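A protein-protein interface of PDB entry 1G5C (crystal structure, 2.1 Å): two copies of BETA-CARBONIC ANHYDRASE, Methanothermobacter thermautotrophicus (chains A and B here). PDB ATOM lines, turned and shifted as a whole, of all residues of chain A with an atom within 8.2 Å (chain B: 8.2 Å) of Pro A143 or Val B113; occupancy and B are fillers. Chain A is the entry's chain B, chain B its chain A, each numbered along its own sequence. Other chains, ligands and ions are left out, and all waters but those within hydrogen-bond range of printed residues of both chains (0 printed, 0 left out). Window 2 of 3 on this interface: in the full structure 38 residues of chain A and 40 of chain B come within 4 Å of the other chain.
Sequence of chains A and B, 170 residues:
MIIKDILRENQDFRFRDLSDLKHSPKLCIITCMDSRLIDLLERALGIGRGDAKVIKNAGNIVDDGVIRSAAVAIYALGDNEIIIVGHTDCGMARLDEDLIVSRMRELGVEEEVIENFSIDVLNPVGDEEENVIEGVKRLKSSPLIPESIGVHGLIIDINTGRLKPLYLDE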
ATOM      1  N   ILE A  67     -18.214   1.498  21.433  1.00  0.00           N
ATOM      2  CA  ILE A  67     -19.226   0.619  20.852  1.00  0.00           C
ATOM      3  C   ILE A  67     -19.027  -0.829  21.306  1.00  0.00           C
ATOM      4  O   ILE A  67     -19.991  -1.532  21.627  1.00  0.00           O
ATOM      5  CB  ILE A  67     -19.201   0.721  19.291  1.00  0.00           C
ATOM      6  CG1 ILE A  67     -19.674   2.124  18.879  1.00  0.00           C
ATOM      7  CG2 ILE A  67     -20.089  -0.360  18.652  1.00  0.00           C
ATOM      8  CD1 ILE A  67     -19.560   2.430  17.390  1.00  0.00           C
ATOM      9  N   ALA A  71     -21.602  -2.971  23.392  1.00  0.00           N
ATOM     10  CA  ALA A  71     -22.045  -4.269  22.874  1.00  0.00           C
ATOM     11  C   ALA A  71     -21.905  -5.349  23.954  1.00  0.00           C
ATOM     12  O   ALA A  71     -22.761  -6.214  24.097  1.00  0.00           O
ATOM     13  CB  ALA A  71     -21.232  -4.642  21.655  1.00  0.00           C
ATOM     14  N   TYR A  75     -25.108  -7.628  25.115  1.00  0.00           N
ATOM     15  CA  TYR A  75     -25.161  -9.073  24.910  1.00  0.00           C
ATOM     16  C   TYR A  75     -24.755  -9.973  26.066  1.00  0.00           C
ATOM     17  O   TYR A  75     -25.047 -11.162  26.051  1.00  0.00           O
ATOM     18  CB  TYR A  75     -24.320  -9.464  23.696  1.00  0.00           C
ATOM     19  CG  TYR A  75     -24.885  -8.966  22.392  1.00  0.00           C
ATOM     20  CD1 TYR A  75     -24.332  -7.863  21.754  1.00  0.00           C
ATOM     21  CD2 TYR A  75     -26.007  -9.572  21.815  1.00  0.00           C
ATOM     22  CE1 TYR A  75     -24.875  -7.367  20.577  1.00  0.00           C
ATOM     23  CE2 TYR A  75     -26.561  -9.081  20.633  1.00  0.00           C
ATOM     24  CZ  TYR A  75     -25.984  -7.977  20.024  1.00  0.00           C
ATOM     25  OH  TYR A  75     -26.510  -7.478  18.855  1.00  0.00           O
ATOM     26  N   ARG A 138     -24.103   7.187  15.651  1.00  0.00           N
ATOM     27  CA  ARG A 138     -23.120   6.130  15.490  1.00  0.00           C
ATOM     28  C   ARG A 138     -23.615   4.848  16.150  1.00  0.00           C
ATOM     29  O   ARG A 138     -23.464   3.756  15.589  1.00  0.00           O
ATOM     30  CB  ARG A 138     -21.774   6.551  16.079  1.00  0.00           C
ATOM     31  CG  ARG A 138     -21.107   7.673  15.316  1.00  0.00           C
ATOM     32  CD  ARG A 138     -19.680   7.942  15.814  1.00  0.00           C
ATOM     33  NE  ARG A 138     -18.983   8.919  14.976  1.00  0.00           N
ATOM     34  CZ  ARG A 138     -17.739   9.343  15.189  1.00  0.00           C
ATOM     35  NH1 ARG A 138     -17.033   8.876  16.218  1.00  0.00           N
ATOM     36  NH2 ARG A 138     -17.205  10.257  14.387  1.00  0.00           N
ATOM     37  N   LEU A 139     -24.223   4.970  17.326  1.00  0.00           N
ATOM     38  CA  LEU A 139     -24.721   3.786  18.010  1.00  0.00           C
ATOM     39  C   LEU A 139     -25.955   3.228  17.297  1.00  0.00           C
ATOM     40  O   LEU A 139     -26.093   2.016  17.140  1.00  0.00           O
ATOM     41  CB  LEU A 139     -25.084   4.095  19.459  1.00  0.00           C
ATOM     42  CG  LEU A 139     -23.977   4.261  20.506  1.00  0.00           C
ATOM     43  CD1 LEU A 139     -24.588   4.827  21.792  1.00  0.00           C
ATOM     44  CD2 LEU A 139     -23.288   2.914  20.752  1.00  0.00           C
ATOM     45  N   LYS A 140     -26.847   4.120  16.881  1.00  0.00           N
ATOM     46  CA  LYS A 140     -28.066   3.725  16.195  1.00  0.00           C
ATOM     47  C   LYS A 140     -27.775   3.015  14.880  1.00  0.00           C
ATOM     48  O   LYS A 140     -28.528   2.144  14.463  1.00  0.00           O
ATOM     49  CB  LYS A 140     -28.930   4.949  15.916  1.00  0.00           C
ATOM     50  CG  LYS A 140     -29.722   5.464  17.102  1.00  0.00           C
ATOM     51  CD  LYS A 140     -31.011   4.701  17.240  1.00  0.00           C
ATOM     52  CE  LYS A 140     -32.077   5.561  17.876  1.00  0.00           C
ATOM     53  NZ  LYS A 140     -33.357   4.821  17.990  1.00  0.00           N
ATOM     54  N   SER A 141     -26.685   3.387  14.219  1.00  0.00           N
ATOM     55  CA  SER A 141     -26.350   2.767  12.948  1.00  0.00           C
ATOM     56  C   SER A 141     -25.337   1.635  13.054  1.00  0.00           C
ATOM     57  O   SER A 141     -24.927   1.080  12.037  1.00  0.00           O
ATOM     58  CB  SER A 141     -25.828   3.819  11.968  1.00  0.00           C
ATOM     59  OG  SER A 141     -24.620   4.392  12.427  1.00  0.00           O
ATOM     60  N   SER A 142     -24.924   1.286  14.268  1.00  0.00           N
ATOM     61  CA  SER A 142     -23.952   0.199  14.425  1.00  0.00           C
ATOM     62  C   SER A 142     -24.622  -1.169  14.398  1.00  0.00           C
ATOM     63  O   SER A 142     -25.623  -1.392  15.075  1.00  0.00           O
ATOM     64  CB  SER A 142     -23.180   0.332  15.740  1.00  0.00           C
ATOM     65  OG  SER A 142     -22.439  -0.856  15.997  1.00  0.00           O
ATOM     66  N   PRO A 143     -24.068  -2.105  13.612  1.00  0.00           N
ATOM     67  CA  PRO A 143     -24.601  -3.468  13.488  1.00  0.00           C
ATOM     68  C   PRO A 143     -24.560  -4.229  14.815  1.00  0.00           C
ATOM     69  O   PRO A 143     -25.345  -5.154  15.036  1.00  0.00           O
ATOM     70  CB  PRO A 143     -23.685  -4.105  12.443  1.00  0.00           C
ATOM     71  CG  PRO A 143     -23.254  -2.950  11.617  1.00  0.00           C
ATOM     72  CD  PRO A 143     -22.982  -1.882  12.644  1.00  0.00           C
ATOM     73  N   LEU A 144     -23.637  -3.827  15.691  1.00  0.00           N
ATOM     74  CA  LEU A 144     -23.451  -4.453  16.997  1.00  0.00           C
ATOM     75  C   LEU A 144     -24.474  -3.996  18.023  1.00  0.00           C
ATOM     76  O   LEU A 144     -24.539  -4.534  19.131  1.00  0.00           O
ATOM     77  CB  LEU A 144     -22.051  -4.144  17.527  1.00  0.00           C
ATOM     78  CG  LEU A 144     -20.864  -4.804  16.827  1.00  0.00           C
ATOM     79  CD1 LEU A 144     -19.545  -4.227  17.340  1.00  0.00           C
ATOM     80  CD2 LEU A 144     -20.929  -6.303  17.069  1.00  0.00           C
ATOM     81  N   ILE A 145     -25.264  -2.992  17.666  1.00  0.00           N
ATOM     82  CA  ILE A 145     -26.275  -2.472  18.580  1.00  0.00           C
ATOM     83  C   ILE A 145     -27.668  -2.792  18.075  1.00  0.00           C
ATOM     84  O   ILE A 145     -28.093  -2.251  17.065  1.00  0.00           O
ATOM     85  CB  ILE A 145     -26.161  -0.942  18.717  1.00  0.00           C
ATOM     86  CG1 ILE A 145     -24.721  -0.561  19.076  1.00  0.00           C
ATOM     87  CG2 ILE A 145     -27.165  -0.440  19.737  1.00  0.00           C
ATOM     88  CD1 ILE A 145     -24.252  -1.102  20.409  1.00  0.00           C
ATOM     89  N   PRO A 146     -28.392  -3.688  18.769  1.00  0.00           N
ATOM     90  CA  PRO A 146     -29.748  -4.061  18.369  1.00  0.00           C
ATOM     91  C   PRO A 146     -30.657  -2.856  18.209  1.00  0.00           C
ATOM     92  O   PRO A 146     -30.668  -1.941  19.043  1.00  0.00           O
ATOM     93  CB  PRO A 146     -30.188  -4.982  19.497  1.00  0.00           C
ATOM     94  CG  PRO A 146     -28.945  -5.729  19.777  1.00  0.00           C
ATOM     95  CD  PRO A 146     -27.887  -4.626  19.790  1.00  0.00           C
ATOM     96  N   GLU A 147     -31.424  -2.854  17.127  1.00  0.00           N
ATOM     97  CA  GLU A 147     -32.340  -1.756  16.866  1.00  0.00           C
ATOM     98  C   GLU A 147     -33.343  -1.588  18.014  1.00  0.00           C
ATOM     99  O   GLU A 147     -33.982  -0.549  18.119  1.00  0.00           O
ATOM    100  CB  GLU A 147     -33.071  -1.993  15.535  1.00  0.00           C
ATOM    101  CG  GLU A 147     -32.140  -2.254  14.334  1.00  0.00           C
ATOM    102  CD  GLU A 147     -31.303  -1.042  13.924  1.00  0.00           C
ATOM    103  OE1 GLU A 147     -31.448   0.040  14.536  1.00  0.00           O
ATOM    104  OE2 GLU A 147     -30.497  -1.174  12.978  1.00  0.00           O
ATOM    105  N   MET B 104     -26.511 -12.694  19.285  1.00  0.00           N
ATOM    106  CA  MET B 104     -26.261 -11.844  18.128  1.00  0.00           C
ATOM    107  C   MET B 104     -26.830 -12.520  16.886  1.00  0.00           C
ATOM    108  O   MET B 104     -27.537 -11.905  16.085  1.00  0.00           O
ATOM    109  CB  MET B 104     -24.761 -11.631  17.946  1.00  0.00           C
ATOM    110  CG  MET B 104     -24.076 -10.981  19.134  1.00  0.00           C
ATOM    111  SD  MET B 104     -22.290 -10.908  18.905  1.00  0.00           S
ATOM    112  CE  MET B 104     -22.137  -9.451  17.908  1.00  0.00           C
ATOM    113  N   LEU B 107     -30.556 -12.027  16.732  1.00  0.00           N
ATOM    114  CA  LEU B 107     -31.075 -10.766  16.212  1.00  0.00           C
ATOM    115  C   LEU B 107     -30.669 -10.535  14.761  1.00  0.00           C
ATOM    116  O   LEU B 107     -30.851  -9.446  14.221  1.00  0.00           O
ATOM    117  CB  LEU B 107     -30.597  -9.597  17.075  1.00  0.00           C
ATOM    118  CG  LEU B 107     -31.235  -9.458  18.462  1.00  0.00           C
ATOM    119  CD1 LEU B 107     -32.746  -9.383  18.325  1.00  0.00           C
ATOM    120  CD2 LEU B 107     -30.850 -10.632  19.336  1.00  0.00           C
ATOM    121  N   GLY B 108     -30.108 -11.562  14.137  1.00  0.00           N
ATOM    122  CA  GLY B 108     -29.713 -11.449  12.746  1.00  0.00           C
ATOM    123  C   GLY B 108     -28.425 -10.698  12.470  1.00  0.00           C
ATOM    124  O   GLY B 108     -28.166 -10.330  11.323  1.00  0.00           O
ATOM    125  N   VAL B 109     -27.612 -10.467  13.497  1.00  0.00           N
ATOM    126  CA  VAL B 109     -26.351  -9.762  13.301  1.00  0.00           C
ATOM    127  C   VAL B 109     -25.546 -10.491  12.237  1.00  0.00           C
ATOM    128  O   VAL B 109     -25.357 -11.703  12.315  1.00  0.00           O
ATOM    129  CB  VAL B 109     -25.517  -9.709  14.598  1.00  0.00           C
ATOM    130  CG1 VAL B 109     -24.181  -9.029  14.331  1.00  0.00           C
ATOM    131  CG2 VAL B 109     -26.282  -8.967  15.678  1.00  0.00           C
ATOM    132  N   GLU B 110     -25.076  -9.748  11.242  1.00  0.00           N
ATOM    133  CA  GLU B 110     -24.292 -10.331  10.158  1.00  0.00           C
ATOM    134  C   GLU B 110     -23.141 -11.168  10.705  1.00  0.00           C
ATOM    135  O   GLU B 110     -22.430 -10.739  11.615  1.00  0.00           O
ATOM    136  CB  GLU B 110     -23.743  -9.223   9.249  1.00  0.00           C
ATOM    137  N   GLU B 111     -22.962 -12.364  10.147  1.00  0.00           N
ATOM    138  CA  GLU B 111     -21.898 -13.257  10.590  1.00  0.00           C
ATOM    139  C   GLU B 111     -20.540 -12.575  10.540  1.00  0.00           C
ATOM    140  O   GLU B 111     -19.700 -12.787  11.414  1.00  0.00           O
ATOM    141  CB  GLU B 111     -21.872 -14.524   9.731  1.00  0.00           C
ATOM    142  CG  GLU B 111     -23.018 -15.494  10.007  1.00  0.00           C
ATOM    143  CD  GLU B 111     -22.953 -16.105  11.399  1.00  0.00           C
ATOM    144  OE1 GLU B 111     -21.946 -16.774  11.718  1.00  0.00           O
ATOM    145  OE2 GLU B 111     -23.912 -15.919  12.175  1.00  0.00           O
ATOM    146  N   GLU B 112     -20.329 -11.753   9.516  1.00  0.00           N
ATOM    147  CA  GLU B 112     -19.066 -11.041   9.364  1.00  0.00           C
ATOM    148  C   GLU B 112     -18.821 -10.210  10.624  1.00  0.00           C
ATOM    149  O   GLU B 112     -17.745 -10.262  11.215  1.00  0.00           O
ATOM    150  N   VAL B 113     -19.841  -9.463  11.033  1.00  0.00           N
ATOM    151  CA  VAL B 113     -19.757  -8.625  12.221  1.00  0.00           C
ATOM    152  C   VAL B 113     -19.467  -9.466  13.464  1.00  0.00           C
ATOM    153  O   VAL B 113     -18.533  -9.178  14.218  1.00  0.00           O
ATOM    154  CB  VAL B 113     -21.071  -7.848  12.437  1.00  0.00           C
ATOM    155  CG1 VAL B 113     -20.984  -7.011  13.702  1.00  0.00           C
ATOM    156  CG2 VAL B 113     -21.350  -6.964  11.236  1.00  0.00           C
ATOM    157  N   ILE B 114     -20.270 -10.507  13.668  1.00  0.00           N
ATOM    158  CA  ILE B 114     -20.106 -11.391  14.817  1.00  0.00           C
ATOM    159  C   ILE B 114     -18.672 -11.905  14.923  1.00  0.00           C
ATOM    160  O   ILE B 114     -18.062 -11.866  15.992  1.00  0.00           O
ATOM    161  CB  ILE B 114     -21.067 -12.598  14.719  1.00  0.00           C
ATOM    162  CG1 ILE B 114     -22.513 -12.096  14.651  1.00  0.00           C
ATOM    163  CG2 ILE B 114     -20.873 -13.524  15.917  1.00  0.00           C
ATOM    164  CD1 ILE B 114     -23.530 -13.177  14.380  1.00  0.00           C
ATOM    165  N   GLU B 115     -18.133 -12.374  13.805  1.00  0.00           N
ATOM    166  CA  GLU B 115     -16.773 -12.897  13.776  1.00  0.00           C
ATOM    167  C   GLU B 115     -15.757 -11.847  14.230  1.00  0.00           C
ATOM    168  O   GLU B 115     -14.854 -12.143  15.014  1.00  0.00           O
ATOM    169  CB  GLU B 115     -16.433 -13.375  12.366  1.00  0.00           C
ATOM    170  CG  GLU B 115     -15.165 -14.202  12.281  1.00  0.00           C
ATOM    171  CD  GLU B 115     -14.884 -14.688  10.874  1.00  0.00           C
ATOM    172  OE1 GLU B 115     -15.785 -15.312  10.269  1.00  0.00           O
ATOM    173  OE2 GLU B 115     -13.761 -14.452  10.375  1.00  0.00           O
ATOM    174  N   ASN B 116     -15.908 -10.622  13.735  1.00  0.00           N
ATOM    175  CA  ASN B 116     -15.009  -9.529  14.098  1.00  0.00           C
ATOM    176  C   ASN B 116     -15.071  -9.293  15.604  1.00  0.00           C
ATOM    177  O   ASN B 116     -14.042  -9.172  16.274  1.00  0.00           O
ATOM    178  CB  ASN B 116     -15.407  -8.243  13.365  1.00  0.00           C
ATOM    179  CG  ASN B 116     -15.366  -8.391  11.855  1.00  0.00           C
ATOM    180  N   PHE B 117     -16.290  -9.225  16.129  1.00  0.00           N
ATOM    181  CA  PHE B 117     -16.497  -9.005  17.548  1.00  0.00           C
ATOM    182  C   PHE B 117     -15.732 -10.068  18.328  1.00  0.00           C
ATOM    183  O   PHE B 117     -14.982  -9.752  19.254  1.00  0.00           O
ATOM    184  CB  PHE B 117     -17.992  -9.082  17.875  1.00  0.00           C
ATOM    185  CG  PHE B 117     -18.343  -8.602  19.259  1.00  0.00           C
ATOM    186  CD1 PHE B 117     -18.107  -7.282  19.634  1.00  0.00           C
ATOM    187  CD2 PHE B 117     -18.924  -9.463  20.182  1.00  0.00           C
ATOM    188  CE1 PHE B 117     -18.450  -6.823  20.903  1.00  0.00           C
ATOM    189  CE2 PHE B 117     -19.272  -9.011  21.459  1.00  0.00           C
ATOM    190  CZ  PHE B 117     -19.030  -7.686  21.815  1.00  0.00           C
ATOM    191  N   SER B 118     -15.915 -11.326  17.930  1.00  0.00           N
ATOM    192  CA  SER B 118     -15.259 -12.459  18.582  1.00  0.00           C
ATOM    193  C   SER B 118     -13.750 -12.310  18.731  1.00  0.00           C
ATOM    194  O   SER B 118     -13.202 -12.482  19.823  1.00  0.00           O
ATOM    195  CB  SER B 118     -15.560 -13.755  17.825  1.00  0.00           C
ATOM    196  OG  SER B 118     -16.929 -14.104  17.934  1.00  0.00           O
ATOM    197  N   ILE B 119     -13.076 -11.987  17.634  1.00  0.00           N
ATOM    198  CA  ILE B 119     -11.627 -11.842  17.662  1.00  0.00           C
ATOM    199  C   ILE B 119     -11.180 -10.583  18.393  1.00  0.00           C
ATOM    200  O   ILE B 119     -10.124 -10.568  19.029  1.00  0.00           O
ATOM    201  CB  ILE B 119     -11.039 -11.820  16.228  1.00  0.00           C
ATOM    202  N   ASP B 120     -11.988  -9.532  18.317  1.00  0.00           N
ATOM    203  CA  ASP B 120     -11.646  -8.262  18.949  1.00  0.00           C
ATOM    204  C   ASP B 120     -11.905  -8.148  20.445  1.00  0.00           C
ATOM    205  O   ASP B 120     -11.119  -7.526  21.162  1.00  0.00           O
ATOM    206  CB  ASP B 120     -12.370  -7.113  18.243  1.00  0.00           C
ATOM    207  CG  ASP B 120     -11.866  -6.887  16.834  1.00  0.00           C
ATOM    208  OD1 ASP B 120     -10.641  -6.723  16.664  1.00  0.00           O
ATOM    209  OD2 ASP B 120     -12.693  -6.868  15.900  1.00  0.00           O
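Among the printed residues, merely in contact across the chains: Leu A144 with Val B113 (3.4 Å), Tyr A75 with Met B104 (3.5 Å), Leu A144 with Met B104 (3.5 Å), Tyr A75 with Val B109 (3.5 Å), Ala A71 with Phe B117 (3.6 Å), Pro A143 with Val B113 (3.9 Å), Leu A144 with Phe B117 (3.9 Å) and Pro A143 with Val B109 (3.98 Å).
Hydrophobic or aromatic side chains of chain B that line the printed part of chain A: Met B104, Val B109, Val B113 and Phe B117. Among the printed residues, 8 pairs touch across the chains.
Ser A142 touches none of the printed residues of chain B. Printed residues of chain B within 4 Å of Leu A144: Met B104 (3.5 Å), Val B113 (3.4 Å) and Phe B117 (3.9 Å). Pro A146 touches none of the printed residues of chain B. Of the printed residues of chain A, Met B104 touches Tyr A75 and Leu A144. Of the printed residues of chain A, Val B109 touches Tyr A75 (3.5 Å) and Pro A143 (3.98 Å). Glu B112 touches none of the printed residues of chain A. Of the printed residues of chain A, Phe B117 touches Ala A71 (3.6 Å) and Leu A144 (3.9 Å). The nearest residue of chain A that does not touch Val B113 is Ser A142 (6.7 Å). The nearest printed residue of chain B that does not touch Tyr A75 is Leu B107 (4.7 Å).
No position is printed for both chains. Of the 8 pairs that touch across the chains among the printed residues, none has its exchanged pair printed and touching as well.
The side-chain hydroxyl (OG) of Ser A142 sits close to the backbone NH (N) of Leu A144, 3.2 Å away. The backbone NH (N) of Val B109 lies within hydrogen-bond range of the backbone carbonyl oxygen (O) of Met B104 (3.0 Å).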
